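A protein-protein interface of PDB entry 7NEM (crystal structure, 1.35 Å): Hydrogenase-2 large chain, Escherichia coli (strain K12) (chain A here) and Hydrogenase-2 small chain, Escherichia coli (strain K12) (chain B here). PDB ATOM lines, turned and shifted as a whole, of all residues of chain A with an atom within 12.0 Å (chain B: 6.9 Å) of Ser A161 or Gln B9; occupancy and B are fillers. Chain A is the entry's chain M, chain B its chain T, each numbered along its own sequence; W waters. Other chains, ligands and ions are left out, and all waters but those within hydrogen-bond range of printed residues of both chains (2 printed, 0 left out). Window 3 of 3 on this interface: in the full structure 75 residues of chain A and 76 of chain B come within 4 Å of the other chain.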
ATOM      1  N   LEU A 123      22.201 -24.749   9.992  1.00  0.00           N
ATOM      2  CA  LEU A 123      23.357 -25.627  10.291  1.00  0.00           C
ATOM      3  C   LEU A 123      23.311 -26.120  11.736  1.00  0.00           C
ATOM      4  O   LEU A 123      23.875 -27.208  11.996  1.00  0.00           O
ATOM      5  CB  LEU A 123      24.667 -24.892  10.022  1.00  0.00           C
ATOM      6  CG  LEU A 123      24.970 -24.634   8.550  1.00  0.00           C
ATOM      7  CD1 LEU A 123      26.246 -23.817   8.426  1.00  0.00           C
ATOM      8  CD2 LEU A 123      25.073 -25.952   7.777  1.00  0.00           C
ATOM      9  N   GLN A 152      20.749 -30.399   4.891  1.00  0.00           N
ATOM     10  CA  GLN A 152      21.717 -29.725   5.797  1.00  0.00           C
ATOM     11  C   GLN A 152      23.140 -29.941   5.289  1.00  0.00           C
ATOM     12  O   GLN A 152      23.933 -28.997   5.298  1.00  0.00           O
ATOM     13  CB  GLN A 152      21.507 -30.245   7.209  1.00  0.00           C
ATOM     14  CG  GLN A 152      22.363 -29.519   8.239  1.00  0.00           C
ATOM     15  CD  GLN A 152      22.118 -30.046   9.636  1.00  0.00           C
ATOM     16  OE1 GLN A 152      22.328 -31.231   9.941  1.00  0.00           O
ATOM     17  NE2 GLN A 152      21.592 -29.168  10.485  1.00  0.00           N
ATOM     18  N   ASN A 153      23.457 -31.147   4.831  1.00  0.00           N
ATOM     19  CA  ASN A 153      24.803 -31.442   4.250  1.00  0.00           C
ATOM     20  C   ASN A 153      25.078 -30.617   2.988  1.00  0.00           C
ATOM     21  O   ASN A 153      26.204 -30.199   2.792  1.00  0.00           O
ATOM     22  CB  ASN A 153      24.993 -32.930   3.979  1.00  0.00           C
ATOM     23  CG  ASN A 153      25.121 -33.724   5.261  1.00  0.00           C
ATOM     24  OD1 ASN A 153      25.428 -33.156   6.312  1.00  0.00           O
ATOM     25  ND2 ASN A 153      24.892 -35.025   5.172  1.00  0.00           N
ATOM     26  N   LYS A 154      24.077 -30.332   2.150  1.00  0.00           N
ATOM     27  CA  LYS A 154      24.335 -29.463   0.975  1.00  0.00           C
ATOM     28  C   LYS A 154      24.674 -28.059   1.486  1.00  0.00           C
ATOM     29  O   LYS A 154      25.540 -27.439   0.890  1.00  0.00           O
ATOM     30  CB  LYS A 154      23.130 -29.354   0.031  1.00  0.00           C
ATOM     31  CG  LYS A 154      22.699 -30.658  -0.606  1.00  0.00           C
ATOM     32  CD  LYS A 154      21.391 -30.463  -1.374  1.00  0.00           C
ATOM     33  CE  LYS A 154      20.794 -31.748  -1.884  1.00  0.00           C
ATOM     34  NZ  LYS A 154      21.464 -32.191  -3.124  1.00  0.00           N
ATOM     35  N   ILE A 155      23.996 -27.570   2.524  1.00  0.00           N
ATOM     36  CA  ILE A 155      24.296 -26.213   3.079  1.00  0.00           C
ATOM     37  C   ILE A 155      25.744 -26.233   3.616  1.00  0.00           C
ATOM     38  O   ILE A 155      26.535 -25.317   3.294  1.00  0.00           O
ATOM     39  CB  ILE A 155      23.339 -25.822   4.219  1.00  0.00           C
ATOM     40  CG1 ILE A 155      21.877 -25.849   3.794  1.00  0.00           C
ATOM     41  CG2 ILE A 155      23.731 -24.447   4.762  1.00  0.00           C
ATOM     42  CD1 ILE A 155      20.926 -25.724   4.968  1.00  0.00           C
ATOM     43  N   LYS A 156      26.044 -27.253   4.419  1.00  0.00           N
ATOM     44  CA  LYS A 156      27.384 -27.488   5.027  1.00  0.00           C
ATOM     45  C   LYS A 156      28.444 -27.410   3.925  1.00  0.00           C
ATOM     46  O   LYS A 156      29.420 -26.631   4.098  1.00  0.00           O
ATOM     47  CB  LYS A 156      27.417 -28.833   5.761  1.00  0.00           C
ATOM     48  CG  LYS A 156      28.422 -28.944   6.897  1.00  0.00           C
ATOM     49  CD  LYS A 156      28.291 -30.235   7.714  1.00  0.00           C
ATOM     50  CE  LYS A 156      26.890 -30.431   8.262  1.00  0.00           C
ATOM     51  NZ  LYS A 156      26.874 -30.898   9.671  1.00  0.00           N
ATOM     52  N   ASP A 157      28.249 -28.122   2.811  1.00  0.00           N
ATOM     53  CA  ASP A 157      29.257 -28.212   1.723  1.00  0.00           C
ATOM     54  C   ASP A 157      29.432 -26.843   1.057  1.00  0.00           C
ATOM     55  O   ASP A 157      30.580 -26.466   0.720  1.00  0.00           O
ATOM     56  CB  ASP A 157      28.864 -29.290   0.713  1.00  0.00           C
ATOM     57  CG  ASP A 157      28.911 -30.706   1.265  1.00  0.00           C
ATOM     58  OD1 ASP A 157      29.530 -30.897   2.312  1.00  0.00           O
ATOM     59  OD2 ASP A 157      28.346 -31.591   0.638  1.00  0.00           O
ATOM     60  N   LEU A 158      28.324 -26.145   0.781  1.00  0.00           N
ATOM     61  CA  LEU A 158      28.402 -24.811   0.159  1.00  0.00           C
ATOM     62  C   LEU A 158      29.200 -23.899   1.103  1.00  0.00           C
ATOM     63  O   LEU A 158      30.136 -23.245   0.602  1.00  0.00           O
ATOM     64  CB  LEU A 158      26.994 -24.274  -0.109  1.00  0.00           C
ATOM     65  CG  LEU A 158      26.978 -22.926  -0.832  1.00  0.00           C
ATOM     66  CD1 LEU A 158      27.091 -23.151  -2.311  1.00  0.00           C
ATOM     67  CD2 LEU A 158      25.730 -22.138  -0.501  1.00  0.00           C
ATOM     68  N   VAL A 159      28.849 -23.848   2.389  1.00  0.00           N
ATOM     69  CA  VAL A 159      29.563 -22.956   3.357  1.00  0.00           C
ATOM     70  C   VAL A 159      31.041 -23.379   3.390  1.00  0.00           C
ATOM     71  O   VAL A 159      31.920 -22.492   3.298  1.00  0.00           O
ATOM     72  CB  VAL A 159      28.902 -22.964   4.753  1.00  0.00           C
ATOM     73  CG1 VAL A 159      29.731 -22.205   5.780  1.00  0.00           C
ATOM     74  CG2 VAL A 159      27.502 -22.394   4.720  1.00  0.00           C
ATOM     75  N   ALA A 160      31.320 -24.679   3.466  1.00  0.00           N
ATOM     76  CA  ALA A 160      32.698 -25.217   3.552  1.00  0.00           C
ATOM     77  C   ALA A 160      33.521 -24.717   2.360  1.00  0.00           C
ATOM     78  O   ALA A 160      34.701 -24.425   2.557  1.00  0.00           O
ATOM     79  CB  ALA A 160      32.701 -26.726   3.649  1.00  0.00           C
ATOM     80  N   SER A 161      32.931 -24.556   1.172  1.00  0.00           N
ATOM     81  CA  SER A 161      33.659 -24.170  -0.062  1.00  0.00           C
ATOM     82  C   SER A 161      34.149 -22.715   0.000  1.00  0.00           C
ATOM     83  O   SER A 161      35.012 -22.400  -0.807  1.00  0.00           O
ATOM     84  CB  SER A 161      32.809 -24.396  -1.298  1.00  0.00           C
ATOM     85  OG  SER A 161      31.830 -23.360  -1.449  1.00  0.00           O
ATOM     86  N   GLY A 162      33.602 -21.886   0.887  1.00  0.00           N
ATOM     87  CA  GLY A 162      33.843 -20.435   0.973  1.00  0.00           C
ATOM     88  C   GLY A 162      33.288 -19.678  -0.224  1.00  0.00           C
ATOM     89  O   GLY A 162      33.611 -18.486  -0.368  1.00  0.00           O
ATOM     90  N   GLN A 163      32.500 -20.332  -1.098  1.00  0.00           N
ATOM     91  CA  GLN A 163      31.872 -19.683  -2.276  1.00  0.00           C
ATOM     92  C   GLN A 163      30.369 -19.650  -2.031  1.00  0.00           C
ATOM     93  O   GLN A 163      29.695 -20.590  -2.449  1.00  0.00           O
ATOM     94  CB  GLN A 163      32.172 -20.416  -3.577  1.00  0.00           C
ATOM     95  CG  GLN A 163      33.621 -20.335  -4.009  1.00  0.00           C
ATOM     96  CD  GLN A 163      33.790 -21.028  -5.333  1.00  0.00           C
ATOM     97  OE1 GLN A 163      33.658 -22.248  -5.409  1.00  0.00           O
ATOM     98  NE2 GLN A 163      34.041 -20.258  -6.364  1.00  0.00           N
ATOM     99  N   LEU A 164      29.877 -18.649  -1.306  1.00  0.00           N
ATOM    100  CA  LEU A 164      28.446 -18.613  -0.919  1.00  0.00           C
ATOM    101  C   LEU A 164      27.630 -18.041  -2.100  1.00  0.00           C
ATOM    102  O   LEU A 164      26.412 -18.320  -2.145  1.00  0.00           O
ATOM    103  CB  LEU A 164      28.312 -17.764   0.341  1.00  0.00           C
ATOM    104  CG  LEU A 164      29.192 -18.193   1.519  1.00  0.00           C
ATOM    105  CD1 LEU A 164      29.081 -17.203   2.686  1.00  0.00           C
ATOM    106  CD2 LEU A 164      28.797 -19.578   1.962  1.00  0.00           C
ATOM    107  N   GLY A 165      28.297 -17.312  -2.994  1.00  0.00           N
ATOM    108  CA  GLY A 165      27.695 -16.690  -4.189  1.00  0.00           C
ATOM    109  C   GLY A 165      26.418 -15.947  -3.820  1.00  0.00           C
ATOM    110  O   GLY A 165      26.454 -15.038  -2.987  1.00  0.00           O
ATOM    111  N   ILE A 166      25.301 -16.341  -4.383  1.00  0.00           N
ATOM    112  CA  ILE A 166      24.004 -15.632  -4.169  1.00  0.00           C
ATOM    113  C   ILE A 166      23.491 -15.800  -2.720  1.00  0.00           C
ATOM    114  O   ILE A 166      22.538 -15.094  -2.353  1.00  0.00           O
ATOM    115  CB  ILE A 166      22.968 -16.100  -5.210  1.00  0.00           C
ATOM    116  CG1 ILE A 166      22.920 -17.623  -5.317  1.00  0.00           C
ATOM    117  CG2 ILE A 166      23.235 -15.432  -6.556  1.00  0.00           C
ATOM    118  CD1 ILE A 166      21.707 -18.145  -6.020  1.00  0.00           C
ATOM    119  N   PHE A 167      24.083 -16.667  -1.891  1.00  0.00           N
ATOM    120  CA  PHE A 167      23.723 -16.783  -0.452  1.00  0.00           C
ATOM    121  C   PHE A 167      24.624 -15.865   0.406  1.00  0.00           C
ATOM    122  O   PHE A 167      24.409 -15.725   1.634  1.00  0.00           O
ATOM    123  CB  PHE A 167      23.720 -18.260  -0.062  1.00  0.00           C
ATOM    124  CG  PHE A 167      22.808 -19.057  -0.952  1.00  0.00           C
ATOM    125  CD1 PHE A 167      21.435 -18.925  -0.829  1.00  0.00           C
ATOM    126  CD2 PHE A 167      23.309 -19.835  -1.982  1.00  0.00           C
ATOM    127  CE1 PHE A 167      20.583 -19.625  -1.668  1.00  0.00           C
ATOM    128  CE2 PHE A 167      22.457 -20.536  -2.820  1.00  0.00           C
ATOM    129  CZ  PHE A 167      21.095 -20.424  -2.667  1.00  0.00           C
ATOM    130  N   ALA A 168      25.590 -15.197  -0.196  1.00  0.00           N
ATOM    131  CA  ALA A 168      26.627 -14.400   0.530  1.00  0.00           C
ATOM    132  C   ALA A 168      26.047 -13.096   1.058  1.00  0.00           C
ATOM    133  O   ALA A 168      25.254 -12.448   0.334  1.00  0.00           O
ATOM    134  CB  ALA A 168      27.788 -14.045  -0.356  1.00  0.00           C
ATOM    135  N   PRO B   8      35.577 -28.178  -3.052  1.00  0.00           N
ATOM    136  CA  PRO B   8      36.126 -28.037  -4.424  1.00  0.00           C
ATOM    137  C   PRO B   8      35.541 -26.799  -5.136  1.00  0.00           C
ATOM    138  O   PRO B   8      34.329 -26.715  -5.224  1.00  0.00           O
ATOM    139  CB  PRO B   8      35.751 -29.349  -5.132  1.00  0.00           C
ATOM    140  CG  PRO B   8      34.544 -29.874  -4.362  1.00  0.00           C
ATOM    141  CD  PRO B   8      34.667 -29.328  -2.950  1.00  0.00           C
ATOM    142  N   GLN B   9      36.393 -25.886  -5.622  1.00  0.00           N
ATOM    143  CA  GLN B   9      35.978 -24.528  -6.107  1.00  0.00           C
ATOM    144  C   GLN B   9      35.202 -24.632  -7.422  1.00  0.00           C
ATOM    145  O   GLN B   9      35.518 -25.484  -8.246  1.00  0.00           O
ATOM    146  CB  GLN B   9      37.170 -23.584  -6.268  1.00  0.00           C
ATOM    147  CG  GLN B   9      37.898 -23.384  -4.934  1.00  0.00           C
ATOM    148  CD  GLN B   9      37.028 -22.715  -3.892  1.00  0.00           C
ATOM    149  OE1 GLN B   9      36.742 -21.533  -3.969  1.00  0.00           O
ATOM    150  NE2 GLN B   9      36.598 -23.461  -2.893  1.00  0.00           N
ATOM    151  N   ARG B  10      34.180 -23.799  -7.583  1.00  0.00           N
ATOM    152  CA  ARG B  10      33.330 -23.810  -8.799  1.00  0.00           C
ATOM    153  C   ARG B  10      33.619 -22.553  -9.595  1.00  0.00           C
ATOM    154  O   ARG B  10      33.930 -21.492  -9.036  1.00  0.00           O
ATOM    155  CB  ARG B  10      31.867 -23.886  -8.356  1.00  0.00           C
ATOM    156  CG  ARG B  10      31.463 -25.251  -7.814  1.00  0.00           C
ATOM    157  CD  ARG B  10      30.159 -25.257  -7.053  1.00  0.00           C
ATOM    158  NE  ARG B  10      30.358 -24.668  -5.743  1.00  0.00           N
ATOM    159  CZ  ARG B  10      29.756 -23.609  -5.254  1.00  0.00           C
ATOM    160  NH1 ARG B  10      28.771 -22.999  -5.906  1.00  0.00           N
ATOM    161  NH2 ARG B  10      30.043 -23.239  -4.016  1.00  0.00           N
ATOM    162  N   PRO B  11      33.512 -22.631 -10.924  1.00  0.00           N
ATOM    163  CA  PRO B  11      33.794 -21.500 -11.794  1.00  0.00           C
ATOM    164  C   PRO B  11      32.799 -20.363 -11.532  1.00  0.00           C
ATOM    165  O   PRO B  11      31.574 -20.554 -11.502  1.00  0.00           O
ATOM    166  CB  PRO B  11      33.688 -22.015 -13.233  1.00  0.00           C
ATOM    167  CG  PRO B  11      33.268 -23.459 -13.119  1.00  0.00           C
ATOM    168  CD  PRO B  11      33.219 -23.857 -11.665  1.00  0.00           C
ATOM    169  N   GLU B  42      26.455 -26.976  -7.703  1.00  0.00           N
ATOM    170  CA  GLU B  42      27.470 -27.945  -8.193  1.00  0.00           C
ATOM    171  C   GLU B  42      28.266 -27.420  -9.373  1.00  0.00           C
ATOM    172  O   GLU B  42      29.478 -27.589  -9.375  1.00  0.00           O
ATOM    173  CB  GLU B  42      26.831 -29.277  -8.583  1.00  0.00           C
ATOM    174  CG  GLU B  42      25.884 -29.832  -7.545  1.00  0.00           C
ATOM    175  CD  GLU B  42      26.533 -30.420  -6.312  1.00  0.00           C
ATOM    176  OE1 GLU B  42      27.770 -30.541  -6.307  1.00  0.00           O
ATOM    177  OE2 GLU B  42      25.794 -30.744  -5.356  1.00  0.00           O
ATOM    178  N   THR B  43      27.647 -26.862 -10.390  1.00  0.00           N
ATOM    179  CA  THR B  43      28.288 -26.549 -11.690  1.00  0.00           C
ATOM    180  C   THR B  43      29.083 -25.237 -11.606  1.00  0.00           C
ATOM    181  O   THR B  43      30.249 -25.204 -12.083  1.00  0.00           O
ATOM    182  CB  THR B  43      27.271 -26.483 -12.823  1.00  0.00           C
ATOM    183  OG1 THR B  43      26.423 -27.636 -12.750  1.00  0.00           O
ATOM    184  CG2 THR B  43      27.948 -26.392 -14.171  1.00  0.00           C
ATOM    185  N   SER B  45      29.686 -21.193  -9.417  1.00  0.00           N
ATOM    186  CA  SER B  45      29.388 -20.278  -8.308  1.00  0.00           C
ATOM    187  C   SER B  45      28.751 -19.040  -8.916  1.00  0.00           C
ATOM    188  O   SER B  45      29.441 -18.271  -9.604  1.00  0.00           O
ATOM    189  CB  SER B  45      30.623 -19.934  -7.507  1.00  0.00           C
ATOM    190  OG  SER B  45      30.261 -19.120  -6.432  1.00  0.00           O
ATOM    191  N   LYS B  70      38.019 -10.454  -6.568  1.00  0.00           N
ATOM    192  CA  LYS B  70      38.445 -11.824  -6.228  1.00  0.00           C
ATOM    193  C   LYS B  70      38.639 -12.656  -7.507  1.00  0.00           C
ATOM    194  O   LYS B  70      39.579 -13.477  -7.563  1.00  0.00           O
ATOM    195  CB  LYS B  70      37.465 -12.489  -5.267  1.00  0.00           C
ATOM    196  CG  LYS B  70      37.836 -13.906  -4.878  1.00  0.00           C
ATOM    197  CD  LYS B  70      36.967 -14.483  -3.809  1.00  0.00           C
ATOM    198  CE  LYS B  70      37.303 -15.932  -3.547  1.00  0.00           C
ATOM    199  NZ  LYS B  70      36.296 -16.566  -2.660  1.00  0.00           N
ATOM    200  N   TYR B  71      37.743 -12.542  -8.490  1.00  0.00           N
ATOM    201  CA  TYR B  71      37.727 -13.460  -9.648  1.00  0.00           C
ATOM    202  C   TYR B  71      38.142 -12.730 -10.918  1.00  0.00           C
ATOM    203  O   TYR B  71      37.858 -13.229 -12.028  1.00  0.00           O
ATOM    204  CB  TYR B  71      36.336 -14.071  -9.810  1.00  0.00           C
ATOM    205  CG  TYR B  71      35.919 -14.931  -8.652  1.00  0.00           C
ATOM    206  CD1 TYR B  71      36.598 -16.103  -8.350  1.00  0.00           C
ATOM    207  CD2 TYR B  71      34.863 -14.584  -7.843  1.00  0.00           C
ATOM    208  CE1 TYR B  71      36.229 -16.916  -7.294  1.00  0.00           C
ATOM    209  CE2 TYR B  71      34.471 -15.394  -6.800  1.00  0.00           C
ATOM    210  CZ  TYR B  71      35.157 -16.562  -6.511  1.00  0.00           C
ATOM    211  OH  TYR B  71      34.745 -17.367  -5.484  1.00  0.00           O
HETATM  212  O   HOH W   1      28.253 -20.267  -4.771  1.00  0.00           O
HETATM  213  O   HOH W   2      32.791 -24.582  -4.344  1.00  0.00           O
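The backbone NH (N) of Arg B10 lies within hydrogen-bond range of the side-chain amide oxygen (OE1) of Gln A163 (2.7 Å). The side-chain hydroxyl (OG) of Ser A161 sits at hydrogen-bond distance from the guanidinium group (NH2) of Arg B10, 3.1 Å away. The side-chain hydroxyl (OH) of Tyr B71 sits at hydrogen-bond distance from the side-chain amide nitrogen (NE2) of Gln A163 (3.1 Å). The side-chain amide nitrogen (NE2) of Gln B9 sits at hydrogen-bond distance from the backbone carbonyl oxygen (O) of Ser A161 (2.8 Å). The side-chain amide oxygen of Gln A163 lies close to the side-chain amide oxygen of Gln B9 (3.5 Å).
The backbone carbonyl oxygen (O) of Pro B11 sits at hydrogen-bond distance from the backbone NH (N) of Ser B45, 2.9 Å away. O of Leu A158 sits at hydrogen-bond distance from OG of Ser A161. The side-chain hydroxyl (OG) of Ser A161 lies close to the backbone NH (N) of Gln A163 (3.1 Å). The side-chain amino group of Lys B70 lies within hydrogen-bond range of the side-chain hydroxyl of Tyr B71.
Among the printed residues, merely in contact across the chains: Leu A158 with Arg B10 and Gln A163 with Ser B45.
Of chain B, only Gln B9 and Arg B10 come within 4 Å of Ser A161. Ile A166 touches none of the printed residues of chain B. No residue of chain A comes within 4 Å of Pro B8. Gln B9 touches just these residues of chain A: Ser A161 (2.8 Å) and Gln A163 (3.3 Å). Arg B10 touches three residues of chain A. Of the printed residues of chain A, Ser B45 touches Gln A163. Of the printed residues of chain A, Tyr B71 touches Gln A163 (3.1 Å). The nearest residue of chain A that does not touch Gln B9 is Gly A162 (5.1 Å). The nearest printed residue of chain B that does not touch Leu A158 is Ser B45 (6.6 Å).
Printed residues of chain A that touch a printed residue of chain B: Leu A158, Ser A161 and Gln A163. Hydrophobic or aromatic side chains of chain A within 4 Å of the printed part of chain B: Leu A158. Of the 9 printed residues of chain B, 4 touch a printed residue of chain A. Hydrophobic or aromatic side chains of chain B that line the printed part of chain A: Tyr B71. Along chain B the printed residues that touch a printed residue of chain A span positions 9 to 71. Among the printed residues, no Asp or Glu carboxylate lies within 4 Å of a Lys or Arg side-chain nitrogen of the other chain.
Water W2 lies within hydrogen-bond range of OE1 of Gln A163, O of Pro B8, NE of Arg B10 and OG of Ser A161. Water W1 lies within hydrogen-bond range of O of Gln A163 (2.8 Å), OG of Ser B45 (2.8 Å), NH1 of Arg B10 (3.0 Å) and N of Gly A165 (3.4 Å).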
